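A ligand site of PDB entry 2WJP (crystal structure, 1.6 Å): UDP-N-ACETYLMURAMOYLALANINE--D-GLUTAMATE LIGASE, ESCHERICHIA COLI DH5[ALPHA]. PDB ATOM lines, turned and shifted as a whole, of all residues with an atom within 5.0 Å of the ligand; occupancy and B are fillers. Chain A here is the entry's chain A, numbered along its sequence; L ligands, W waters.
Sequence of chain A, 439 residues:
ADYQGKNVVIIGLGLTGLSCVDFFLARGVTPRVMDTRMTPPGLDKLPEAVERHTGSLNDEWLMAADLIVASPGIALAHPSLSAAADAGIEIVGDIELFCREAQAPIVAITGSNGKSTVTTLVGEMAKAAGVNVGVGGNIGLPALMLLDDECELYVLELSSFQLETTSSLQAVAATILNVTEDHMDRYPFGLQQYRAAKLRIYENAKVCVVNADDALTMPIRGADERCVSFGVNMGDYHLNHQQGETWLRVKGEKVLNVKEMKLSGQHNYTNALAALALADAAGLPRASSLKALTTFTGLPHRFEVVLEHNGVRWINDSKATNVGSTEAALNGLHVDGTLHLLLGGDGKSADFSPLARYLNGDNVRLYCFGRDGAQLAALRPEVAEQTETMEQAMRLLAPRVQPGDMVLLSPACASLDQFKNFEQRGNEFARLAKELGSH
CG2 of Ile 11 touches S2 of the ligand, at 3.6 Å. Gly 12 touches the ligand. Ser 71 touches the ligand (OG to C17, 3.2 Å). O of Pro 72 touches C10 of the ligand (3.5 Å). Gly 73 touches the ligand. Phe 161 touches the ligand (CE2 to C9, 3.5 Å). His 183 touches the ligand (CE1 to O4, 3.2 Å). Arg 186 touches the ligand (NH1 to C10, 3.96 Å). OG1 of Thr 321 touches O4 of the ligand (3.996 Å). CB of Ala 414 touches O3 of the ligand (3.3 Å). CD2 of Leu 416 touches C2 of the ligand, at 3.5 Å. CA of Asn 421 touches O1 of the ligand, at 3.3 Å. Hydrophobic or aromatic side chains that line the ligand: Ile 11, Phe 161, His 183, Ala 414, Leu 416 and Phe 422. Within 4 Å of the ligand: Ile 11, Gly 12, Asp 35, Thr 36, Arg 37, Ser 71, Pro 72, Gly 73, Phe 161, His 183, Arg 186, Thr 321, Lys 348, Ala 414, Ser 415, Leu 416, Asn 421 and Phe 422. The nearest printed residue that does not touch the ligand is Ile 74 (4.05 Å).
Water W5 lies within hydrogen-bond range of an oxygen (O4) of the ligand (2.6 Å), the side-chain carboxylate (OD2) of Asp 182 (2.7 Å), the side-chain hydroxyl (OG1) of Thr 321 (2.7 Å) and the side-chain amino group (NZ) of Lys 348 (3.0 Å).
A nitrogen (N3) of the ligand sits at hydrogen-bond distance from the side-chain hydroxyl of Thr 36 (2.8 Å). The backbone NH (N) of Phe 422 sits at hydrogen-bond distance from an oxygen (O1) of the ligand. The side-chain carboxylate (OD1) of Asp 35 is in hydrogen-bond range of a nitrogen (N3) of the ligand, at 3.5 Å. An oxygen (O2) of the ligand sits at hydrogen-bond distance from the side-chain hydroxyl of Ser 415, 2.8 Å away. An oxygen (O2) of the ligand sits at hydrogen-bond distance from the backbone NH (N) of Ser 415 (3.0 Å). A sulfur (S2) of the ligand lies close to the backbone NH (N) of Thr 36, 3.4 Å away. An oxygen (O3) of the ligand lies within salt-bridge range of the side-chain amino group of Lys 348 (2.7 Å). A sulfur (S1) of the ligand sits close to the guanidinium group (NH2) of Arg 37.
The backbone carbonyl oxygen (O) of Met 34 sits at hydrogen-bond distance from the backbone NH (N) of Gly 12 (2.8 Å). The side-chain carboxylate (OD2) of Asp 182 lies within hydrogen-bond range of a ring nitrogen (NE2) of His 183 (3.3 Å). OG of Ser 415 lies close to O of Asn 421 (3.2 Å). NH2 of Arg 186 sits at hydrogen-bond distance from O of Ile 74 (3.3 Å). The backbone NH (N) of Ser 71 lies within hydrogen-bond range of the backbone carbonyl oxygen (O) of Ile 11, at 2.9 Å. The backbone NH of Glu 423 sits close to the side-chain amide oxygen of Asn 421 (3.4 Å). The backbone carbonyl oxygen (O) of Pro 72 is in hydrogen-bond range of the guanidinium group (NH1) of Arg 186 (2.8 Å). OG of Ser 71 sits at hydrogen-bond distance from N of Gly 73 (2.9 Å).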
ATOM      1  N   ILE A  11      25.108  -8.533  -2.367  1.00  0.00           N
ATOM      2  CA  ILE A  11      24.937  -7.455  -1.395  1.00  0.00           C
ATOM      3  C   ILE A  11      23.805  -7.803  -0.432  1.00  0.00           C
ATOM      4  O   ILE A  11      22.635  -7.934  -0.849  1.00  0.00           O
ATOM      5  CB  ILE A  11      24.570  -6.115  -2.067  1.00  0.00           C
ATOM      6  CG1 ILE A  11      25.551  -5.778  -3.203  1.00  0.00           C
ATOM      7  CG2 ILE A  11      24.499  -4.996  -1.010  1.00  0.00           C
ATOM      8  CD1 ILE A  11      25.183  -4.467  -3.948  1.00  0.00           C
ATOM      9  N   GLY A  12      24.140  -7.973   0.844  1.00  0.00           N
ATOM     10  CA  GLY A  12      23.143  -8.286   1.886  1.00  0.00           C
ATOM     11  C   GLY A  12      23.216  -9.752   2.262  1.00  0.00           C
ATOM     12  O   GLY A  12      23.117 -10.642   1.384  1.00  0.00           O
ATOM     13  N   MET A  34      29.143  -8.499   0.370  1.00  0.00           N
ATOM     14  CA  MET A  34      29.221  -7.288   1.198  1.00  0.00           C
ATOM     15  C   MET A  34      27.889  -6.946   1.849  1.00  0.00           C
ATOM     16  O   MET A  34      26.833  -7.326   1.354  1.00  0.00           O
ATOM     17  CB  MET A  34      29.714  -6.099   0.348  1.00  0.00           C
ATOM     18  CG  MET A  34      28.772  -5.708  -0.790  1.00  0.00           C
ATOM     19  SD  MET A  34      29.416  -4.341  -1.814  1.00  0.00           S
ATOM     20  CE  MET A  34      30.845  -5.097  -2.537  1.00  0.00           C
ATOM     21  N   ASP A  35      27.950  -6.199   2.951  1.00  0.00           N
ATOM     22  CA  ASP A  35      26.758  -5.777   3.681  1.00  0.00           C
ATOM     23  C   ASP A  35      27.115  -4.485   4.440  1.00  0.00           C
ATOM     24  O   ASP A  35      28.216  -4.340   4.968  1.00  0.00           O
ATOM     25  CB  ASP A  35      26.363  -6.907   4.650  1.00  0.00           C
ATOM     26  CG  ASP A  35      24.969  -6.763   5.241  1.00  0.00           C
ATOM     27  OD1 ASP A  35      24.672  -5.733   5.886  1.00  0.00           O
ATOM     28  OD2 ASP A  35      24.152  -7.692   5.042  1.00  0.00           O
ATOM     29  N   THR A  36      26.202  -3.519   4.450  1.00  0.00           N
ATOM     30  CA  THR A  36      26.491  -2.255   5.104  1.00  0.00           C
ATOM     31  C   THR A  36      26.513  -2.375   6.630  1.00  0.00           C
ATOM     32  O   THR A  36      27.022  -1.483   7.307  1.00  0.00           O
ATOM     33  CB  THR A  36      25.543  -1.140   4.671  1.00  0.00           C
ATOM     34  OG1 THR A  36      24.227  -1.449   5.142  1.00  0.00           O
ATOM     35  CG2 THR A  36      25.554  -0.983   3.146  1.00  0.00           C
ATOM     36  N   ARG A  37      25.946  -3.451   7.158  1.00  0.00           N
ATOM     37  CA  ARG A  37      26.000  -3.739   8.590  1.00  0.00           C
ATOM     38  C   ARG A  37      27.341  -4.341   9.016  1.00  0.00           C
ATOM     39  O   ARG A  37      27.867  -5.232   8.349  1.00  0.00           O
ATOM     40  CB  ARG A  37      24.823  -4.659   8.960  1.00  0.00           C
ATOM     41  CG  ARG A  37      23.450  -4.045   8.610  1.00  0.00           C
ATOM     42  CD  ARG A  37      22.325  -5.087   8.695  1.00  0.00           C
ATOM     43  NE  ARG A  37      22.359  -6.045   7.582  1.00  0.00           N
ATOM     44  CZ  ARG A  37      21.433  -6.968   7.346  1.00  0.00           C
ATOM     45  NH1 ARG A  37      20.363  -7.089   8.132  1.00  0.00           N
ATOM     46  NH2 ARG A  37      21.565  -7.763   6.294  1.00  0.00           N
ATOM     47  N   LEU A  57      29.504  -0.517   1.743  1.00  0.00           N
ATOM     48  CA  LEU A  57      29.696  -1.144   0.435  1.00  0.00           C
ATOM     49  C   LEU A  57      31.113  -0.915  -0.073  1.00  0.00           C
ATOM     50  O   LEU A  57      31.762   0.035   0.356  1.00  0.00           O
ATOM     51  CB  LEU A  57      28.659  -0.649  -0.589  1.00  0.00           C
ATOM     52  CG  LEU A  57      27.177  -0.868  -0.191  1.00  0.00           C
ATOM     53  CD1 LEU A  57      26.284  -0.541  -1.365  1.00  0.00           C
ATOM     54  CD2 LEU A  57      26.948  -2.337   0.214  1.00  0.00           C
ATOM     55  N   SER A  71      20.210  -7.697  -2.333  1.00  0.00           N
ATOM     56  CA  SER A  71      19.118  -7.955  -1.381  1.00  0.00           C
ATOM     57  C   SER A  71      17.993  -6.950  -1.623  1.00  0.00           C
ATOM     58  O   SER A  71      18.276  -5.794  -1.905  1.00  0.00           O
ATOM     59  CB  SER A  71      19.623  -7.729   0.053  1.00  0.00           C
ATOM     60  OG  SER A  71      18.577  -7.819   1.022  1.00  0.00           O
ATOM     61  N   PRO A  72      16.750  -7.339  -1.355  1.00  0.00           N
ATOM     62  CA  PRO A  72      15.675  -6.322  -1.355  1.00  0.00           C
ATOM     63  C   PRO A  72      15.848  -5.274  -0.253  1.00  0.00           C
ATOM     64  O   PRO A  72      15.191  -4.230  -0.276  1.00  0.00           O
ATOM     65  CB  PRO A  72      14.405  -7.146  -1.125  1.00  0.00           C
ATOM     66  CG  PRO A  72      14.862  -8.423  -0.502  1.00  0.00           C
ATOM     67  CD  PRO A  72      16.212  -8.699  -1.131  1.00  0.00           C
ATOM     68  N   GLY A  73      16.752  -5.533   0.677  1.00  0.00           N
ATOM     69  CA  GLY A  73      16.996  -4.625   1.803  1.00  0.00           C
ATOM     70  C   GLY A  73      17.971  -3.486   1.522  1.00  0.00           C
ATOM     71  O   GLY A  73      18.059  -2.555   2.314  1.00  0.00           O
ATOM     72  N   ILE A  74      18.586  -3.462   0.343  1.00  0.00           N
ATOM     73  CA  ILE A  74      19.470  -2.358  -0.060  1.00  0.00           C
ATOM     74  C   ILE A  74      18.816  -1.567  -1.184  1.00  0.00           C
ATOM     75  O   ILE A  74      18.336  -2.134  -2.168  1.00  0.00           O
ATOM     76  CB  ILE A  74      20.890  -2.862  -0.494  1.00  0.00           C
ATOM     77  CG1 ILE A  74      21.876  -1.710  -0.742  1.00  0.00           C
ATOM     78  CG2 ILE A  74      20.832  -3.780  -1.712  1.00  0.00           C
ATOM     79  CD1 ILE A  74      22.298  -1.043   0.547  1.00  0.00           C
ATOM     80  N   PHE A 161      10.132  -4.504  -3.516  1.00  0.00           N
ATOM     81  CA  PHE A 161      11.599  -4.476  -3.640  1.00  0.00           C
ATOM     82  C   PHE A 161      12.149  -5.646  -4.453  1.00  0.00           C
ATOM     83  O   PHE A 161      13.043  -5.445  -5.294  1.00  0.00           O
ATOM     84  CB  PHE A 161      12.239  -4.425  -2.256  1.00  0.00           C
ATOM     85  CG  PHE A 161      11.699  -3.301  -1.409  1.00  0.00           C
ATOM     86  CD1 PHE A 161      11.889  -1.972  -1.781  1.00  0.00           C
ATOM     87  CD2 PHE A 161      10.972  -3.593  -0.269  1.00  0.00           C
ATOM     88  CE1 PHE A 161      11.345  -0.936  -1.006  1.00  0.00           C
ATOM     89  CE2 PHE A 161      10.481  -2.555   0.538  1.00  0.00           C
ATOM     90  CZ  PHE A 161      10.698  -1.233   0.167  1.00  0.00           C
ATOM     91  N   ASP A 182       2.816   2.772   1.683  1.00  0.00           N
ATOM     92  CA  ASP A 182       3.790   2.028   2.490  1.00  0.00           C
ATOM     93  C   ASP A 182       5.177   2.255   1.879  1.00  0.00           C
ATOM     94  O   ASP A 182       5.312   2.693   0.733  1.00  0.00           O
ATOM     95  CB  ASP A 182       3.442   0.537   2.500  1.00  0.00           C
ATOM     96  CG  ASP A 182       4.130  -0.236   3.639  1.00  0.00           C
ATOM     97  OD1 ASP A 182       4.821   0.380   4.476  1.00  0.00           O
ATOM     98  OD2 ASP A 182       3.924  -1.481   3.689  1.00  0.00           O
ATOM     99  N   HIS A 183       6.211   2.049   2.694  1.00  0.00           N
ATOM    100  CA  HIS A 183       7.596   2.134   2.225  1.00  0.00           C
ATOM    101  C   HIS A 183       7.983   3.464   1.615  1.00  0.00           C
ATOM    102  O   HIS A 183       8.841   3.507   0.756  1.00  0.00           O
ATOM    103  CB  HIS A 183       7.883   0.997   1.237  1.00  0.00           C
ATOM    104  CG  HIS A 183       7.582  -0.366   1.802  1.00  0.00           C
ATOM    105  ND1 HIS A 183       8.282  -0.886   2.869  1.00  0.00           N
ATOM    106  CD2 HIS A 183       6.676  -1.296   1.444  1.00  0.00           C
ATOM    107  CE1 HIS A 183       7.785  -2.075   3.167  1.00  0.00           C
ATOM    108  NE2 HIS A 183       6.826  -2.360   2.300  1.00  0.00           N
ATOM    109  N   ARG A 186      11.495   4.548   1.101  1.00  0.00           N
ATOM    110  CA  ARG A 186      12.253   3.921   0.011  1.00  0.00           C
ATOM    111  C   ARG A 186      11.746   4.272  -1.371  1.00  0.00           C
ATOM    112  O   ARG A 186      12.341   3.846  -2.359  1.00  0.00           O
ATOM    113  CB  ARG A 186      12.330   2.397   0.137  1.00  0.00           C
ATOM    114  CG  ARG A 186      13.195   2.072   1.341  1.00  0.00           C
ATOM    115  CD  ARG A 186      14.039   0.833   1.261  1.00  0.00           C
ATOM    116  NE  ARG A 186      14.519   0.372  -0.021  1.00  0.00           N
ATOM    117  CZ  ARG A 186      14.896  -0.908  -0.174  1.00  0.00           C
ATOM    118  NH1 ARG A 186      14.687  -1.712   0.860  1.00  0.00           N
ATOM    119  NH2 ARG A 186      15.203  -1.412  -1.359  1.00  0.00           N
ATOM    120  N   THR A 321       1.979  -3.642   9.737  1.00  0.00           N
ATOM    121  CA  THR A 321       3.164  -2.782   9.651  1.00  0.00           C
ATOM    122  C   THR A 321       2.913  -1.522   8.814  1.00  0.00           C
ATOM    123  O   THR A 321       3.833  -0.742   8.541  1.00  0.00           O
ATOM    124  CB  THR A 321       4.369  -3.555   9.065  1.00  0.00           C
ATOM    125  OG1 THR A 321       3.947  -4.173   7.835  1.00  0.00           O
ATOM    126  CG2 THR A 321       4.788  -4.686  10.028  1.00  0.00           C
ATOM    127  N   LYS A 348       7.900   4.733   8.644  1.00  0.00           N
ATOM    128  CA  LYS A 348       8.353   4.788   7.223  1.00  0.00           C
ATOM    129  C   LYS A 348       7.819   6.026   6.479  1.00  0.00           C
ATOM    130  O   LYS A 348       7.526   5.979   5.269  1.00  0.00           O
ATOM    131  CB  LYS A 348       7.949   3.508   6.488  1.00  0.00           C
ATOM    132  CG  LYS A 348       8.712   2.254   6.964  1.00  0.00           C
ATOM    133  CD  LYS A 348       8.071   0.936   6.491  1.00  0.00           C
ATOM    134  CE  LYS A 348       6.842   0.639   7.330  1.00  0.00           C
ATOM    135  NZ  LYS A 348       6.099  -0.519   6.815  1.00  0.00           N
ATOM    136  N   ALA A 414       6.611  -0.470  10.967  1.00  0.00           N
ATOM    137  CA  ALA A 414       7.637  -1.481  11.102  1.00  0.00           C
ATOM    138  C   ALA A 414       8.169  -1.557  12.531  1.00  0.00           C
ATOM    139  O   ALA A 414       8.098  -0.589  13.296  1.00  0.00           O
ATOM    140  CB  ALA A 414       8.791  -1.213  10.083  1.00  0.00           C
ATOM    141  N   SER A 415       8.754  -2.710  12.858  1.00  0.00           N
ATOM    142  CA  SER A 415       9.239  -2.981  14.215  1.00  0.00           C
ATOM    143  C   SER A 415      10.755  -2.782  14.305  1.00  0.00           C
ATOM    144  O   SER A 415      11.305  -2.863  15.386  1.00  0.00           O
ATOM    145  CB  SER A 415       8.933  -4.435  14.591  1.00  0.00           C
ATOM    146  OG  SER A 415       9.789  -5.325  13.884  1.00  0.00           O
ATOM    147  N   LEU A 416      11.386  -2.409  13.195  1.00  0.00           N
ATOM    148  CA  LEU A 416      12.841  -2.613  13.067  1.00  0.00           C
ATOM    149  C   LEU A 416      13.664  -1.626  13.897  1.00  0.00           C
ATOM    150  O   LEU A 416      14.871  -1.828  14.091  1.00  0.00           O
ATOM    151  CB  LEU A 416      13.250  -2.582  11.586  1.00  0.00           C
ATOM    152  CG  LEU A 416      12.542  -3.632  10.705  1.00  0.00           C
ATOM    153  CD1 LEU A 416      12.991  -3.588   9.246  1.00  0.00           C
ATOM    154  CD2 LEU A 416      12.681  -5.047  11.289  1.00  0.00           C
ATOM    155  N   ASN A 421      12.245  -8.144  14.144  1.00  0.00           N
ATOM    156  CA  ASN A 421      11.201  -8.282  13.126  1.00  0.00           C
ATOM    157  C   ASN A 421       9.835  -8.277  13.800  1.00  0.00           C
ATOM    158  O   ASN A 421       9.759  -8.317  15.031  1.00  0.00           O
ATOM    159  CB  ASN A 421      11.396  -9.542  12.270  1.00  0.00           C
ATOM    160  CG  ASN A 421      11.625 -10.799  13.113  1.00  0.00           C
ATOM    161  OD1 ASN A 421      10.984 -11.019  14.150  1.00  0.00           O
ATOM    162  ND2 ASN A 421      12.518 -11.643  12.638  1.00  0.00           N
ATOM    163  N   PHE A 422       8.774  -8.247  12.992  1.00  0.00           N
ATOM    164  CA  PHE A 422       7.431  -8.155  13.586  1.00  0.00           C
ATOM    165  C   PHE A 422       7.035  -9.414  14.347  1.00  0.00           C
ATOM    166  O   PHE A 422       6.257  -9.333  15.301  1.00  0.00           O
ATOM    167  CB  PHE A 422       6.370  -7.802  12.531  1.00  0.00           C
ATOM    168  CG  PHE A 422       6.022  -8.952  11.607  1.00  0.00           C
ATOM    169  CD1 PHE A 422       5.079  -9.898  11.990  1.00  0.00           C
ATOM    170  CD2 PHE A 422       6.719  -9.133  10.434  1.00  0.00           C
ATOM    171  CE1 PHE A 422       4.805 -10.998  11.169  1.00  0.00           C
ATOM    172  CE2 PHE A 422       6.466 -10.236   9.607  1.00  0.00           C
ATOM    173  CZ  PHE A 422       5.492 -11.161   9.971  1.00  0.00           C
ATOM    174  N   GLU A 423       7.641 -10.556  14.010  1.00  0.00           N
ATOM    175  CA  GLU A 423       7.401 -11.781  14.780  1.00  0.00           C
ATOM    176  C   GLU A 423       7.896 -11.647  16.212  1.00  0.00           C
ATOM    177  O   GLU A 423       7.225 -12.051  17.170  1.00  0.00           O
ATOM    178  CB  GLU A 423       8.094 -12.969  14.090  1.00  0.00           C
ATOM    179  CG  GLU A 423       7.370 -13.380  12.856  1.00  0.00           C
ATOM    180  CD  GLU A 423       8.003 -12.814  11.616  1.00  0.00           C
ATOM    181  OE1 GLU A 423       8.670 -11.763  11.738  1.00  0.00           O
ATOM    182  OE2 GLU A 423       7.936 -13.477  10.559  1.00  0.00           O
ATOM    183  N   ARG A 425       8.350  -8.837  17.896  1.00  0.00           N
ATOM    184  CA  ARG A 425       7.414  -7.916  18.527  1.00  0.00           C
ATOM    185  C   ARG A 425       6.112  -8.599  18.959  1.00  0.00           C
ATOM    186  O   ARG A 425       5.674  -8.405  20.087  1.00  0.00           O
ATOM    187  CB  ARG A 425       7.115  -6.721  17.599  1.00  0.00           C
ATOM    188  CG  ARG A 425       6.018  -5.769  18.071  1.00  0.00           C
ATOM    189  CD  ARG A 425       5.935  -4.540  17.144  1.00  0.00           C
ATOM    190  NE  ARG A 425       5.378  -4.899  15.840  1.00  0.00           N
ATOM    191  CZ  ARG A 425       5.318  -4.061  14.818  1.00  0.00           C
ATOM    192  NH1 ARG A 425       5.817  -2.819  14.938  1.00  0.00           N
ATOM    193  NH2 ARG A 425       4.754  -4.452  13.675  1.00  0.00           N
HETATM  194  O1  LIG L   1       9.374  -7.265  10.522  1.00  0.00           O
HETATM  195  C1  LIG L   1       9.168  -6.050  10.437  1.00  0.00           C
HETATM  196  O2  LIG L   1       8.637  -5.261  11.282  1.00  0.00           O
HETATM  197  C2  LIG L   1       9.876  -5.479   9.194  1.00  0.00           C
HETATM  198  C3  LIG L   1       9.143  -4.349   8.549  1.00  0.00           C
HETATM  199  C4  LIG L   1       8.952  -4.630   7.057  1.00  0.00           C
HETATM  200  C5  LIG L   1       8.037  -3.600   6.486  1.00  0.00           C
HETATM  201  O3  LIG L   1       7.843  -2.602   7.218  1.00  0.00           O
HETATM  202  O4  LIG L   1       7.278  -4.067   5.630  1.00  0.00           O
HETATM  203  N1  LIG L   1      10.140  -4.902   6.213  1.00  0.00           N
HETATM  204  C6  LIG L   1      10.657  -4.127   5.264  1.00  0.00           C
HETATM  205  O5  LIG L   1      10.492  -2.920   5.132  1.00  0.00           O
HETATM  206  C7  LIG L   1      11.677  -4.843   4.383  1.00  0.00           C
HETATM  207  C8  LIG L   1      12.233  -6.052   4.821  1.00  0.00           C
HETATM  208  C9  LIG L   1      12.035  -4.265   3.175  1.00  0.00           C
HETATM  209  C10 LIG L   1      12.958  -4.940   2.374  1.00  0.00           C
HETATM  210  C11 LIG L   1      13.483  -6.151   2.791  1.00  0.00           C
HETATM  211  C12 LIG L   1      13.149  -6.722   4.014  1.00  0.00           C
HETATM  212  C13 LIG L   1      13.658  -8.099   4.436  1.00  0.00           C
HETATM  213  N2  LIG L   1      15.079  -8.283   4.045  1.00  0.00           N
HETATM  214  C14 LIG L   1      16.070  -7.500   4.490  1.00  0.00           C
HETATM  215  C15 LIG L   1      15.850  -6.522   5.474  1.00  0.00           C
HETATM  216  C16 LIG L   1      16.892  -5.684   5.883  1.00  0.00           C
HETATM  217  C17 LIG L   1      17.356  -7.666   3.969  1.00  0.00           C
HETATM  218  C18 LIG L   1      18.406  -6.858   4.427  1.00  0.00           C
HETATM  219  C19 LIG L   1      18.166  -5.812   5.323  1.00  0.00           C
HETATM  220  C20 LIG L   1      19.179  -4.924   5.722  1.00  0.00           C
HETATM  221  C21 LIG L   1      20.337  -4.595   5.045  1.00  0.00           C
HETATM  222  S1  LIG L   1      20.961  -5.297   3.596  1.00  0.00           S
HETATM  223  C22 LIG L   1      22.389  -4.304   3.552  1.00  0.00           C
HETATM  224  S2  LIG L   1      23.573  -4.398   2.423  1.00  0.00           S
HETATM  225  N3  LIG L   1      22.386  -3.441   4.586  1.00  0.00           N
HETATM  226  C23 LIG L   1      21.255  -3.573   5.422  1.00  0.00           C
HETATM  227  O6  LIG L   1      21.125  -2.822   6.385  1.00  0.00           O
HETATM  228  O   HOH W   1       9.596  -8.049   6.093  1.00  0.00           O
HETATM  229  O   HOH W   2      10.351  -8.455   8.575  1.00  0.00           O
HETATM  230  O   HOH W   3      11.112  -0.684   7.128  1.00  0.00           O
HETATM  231  O   HOH W   4      15.501 -10.628   2.140  1.00  0.00           O
HETATM  232  O   HOH W   5       4.924  -3.056   5.605  1.00  0.00           O
HETATM  233  O   HOH W   6      17.204  -8.102   8.006  1.00  0.00           O
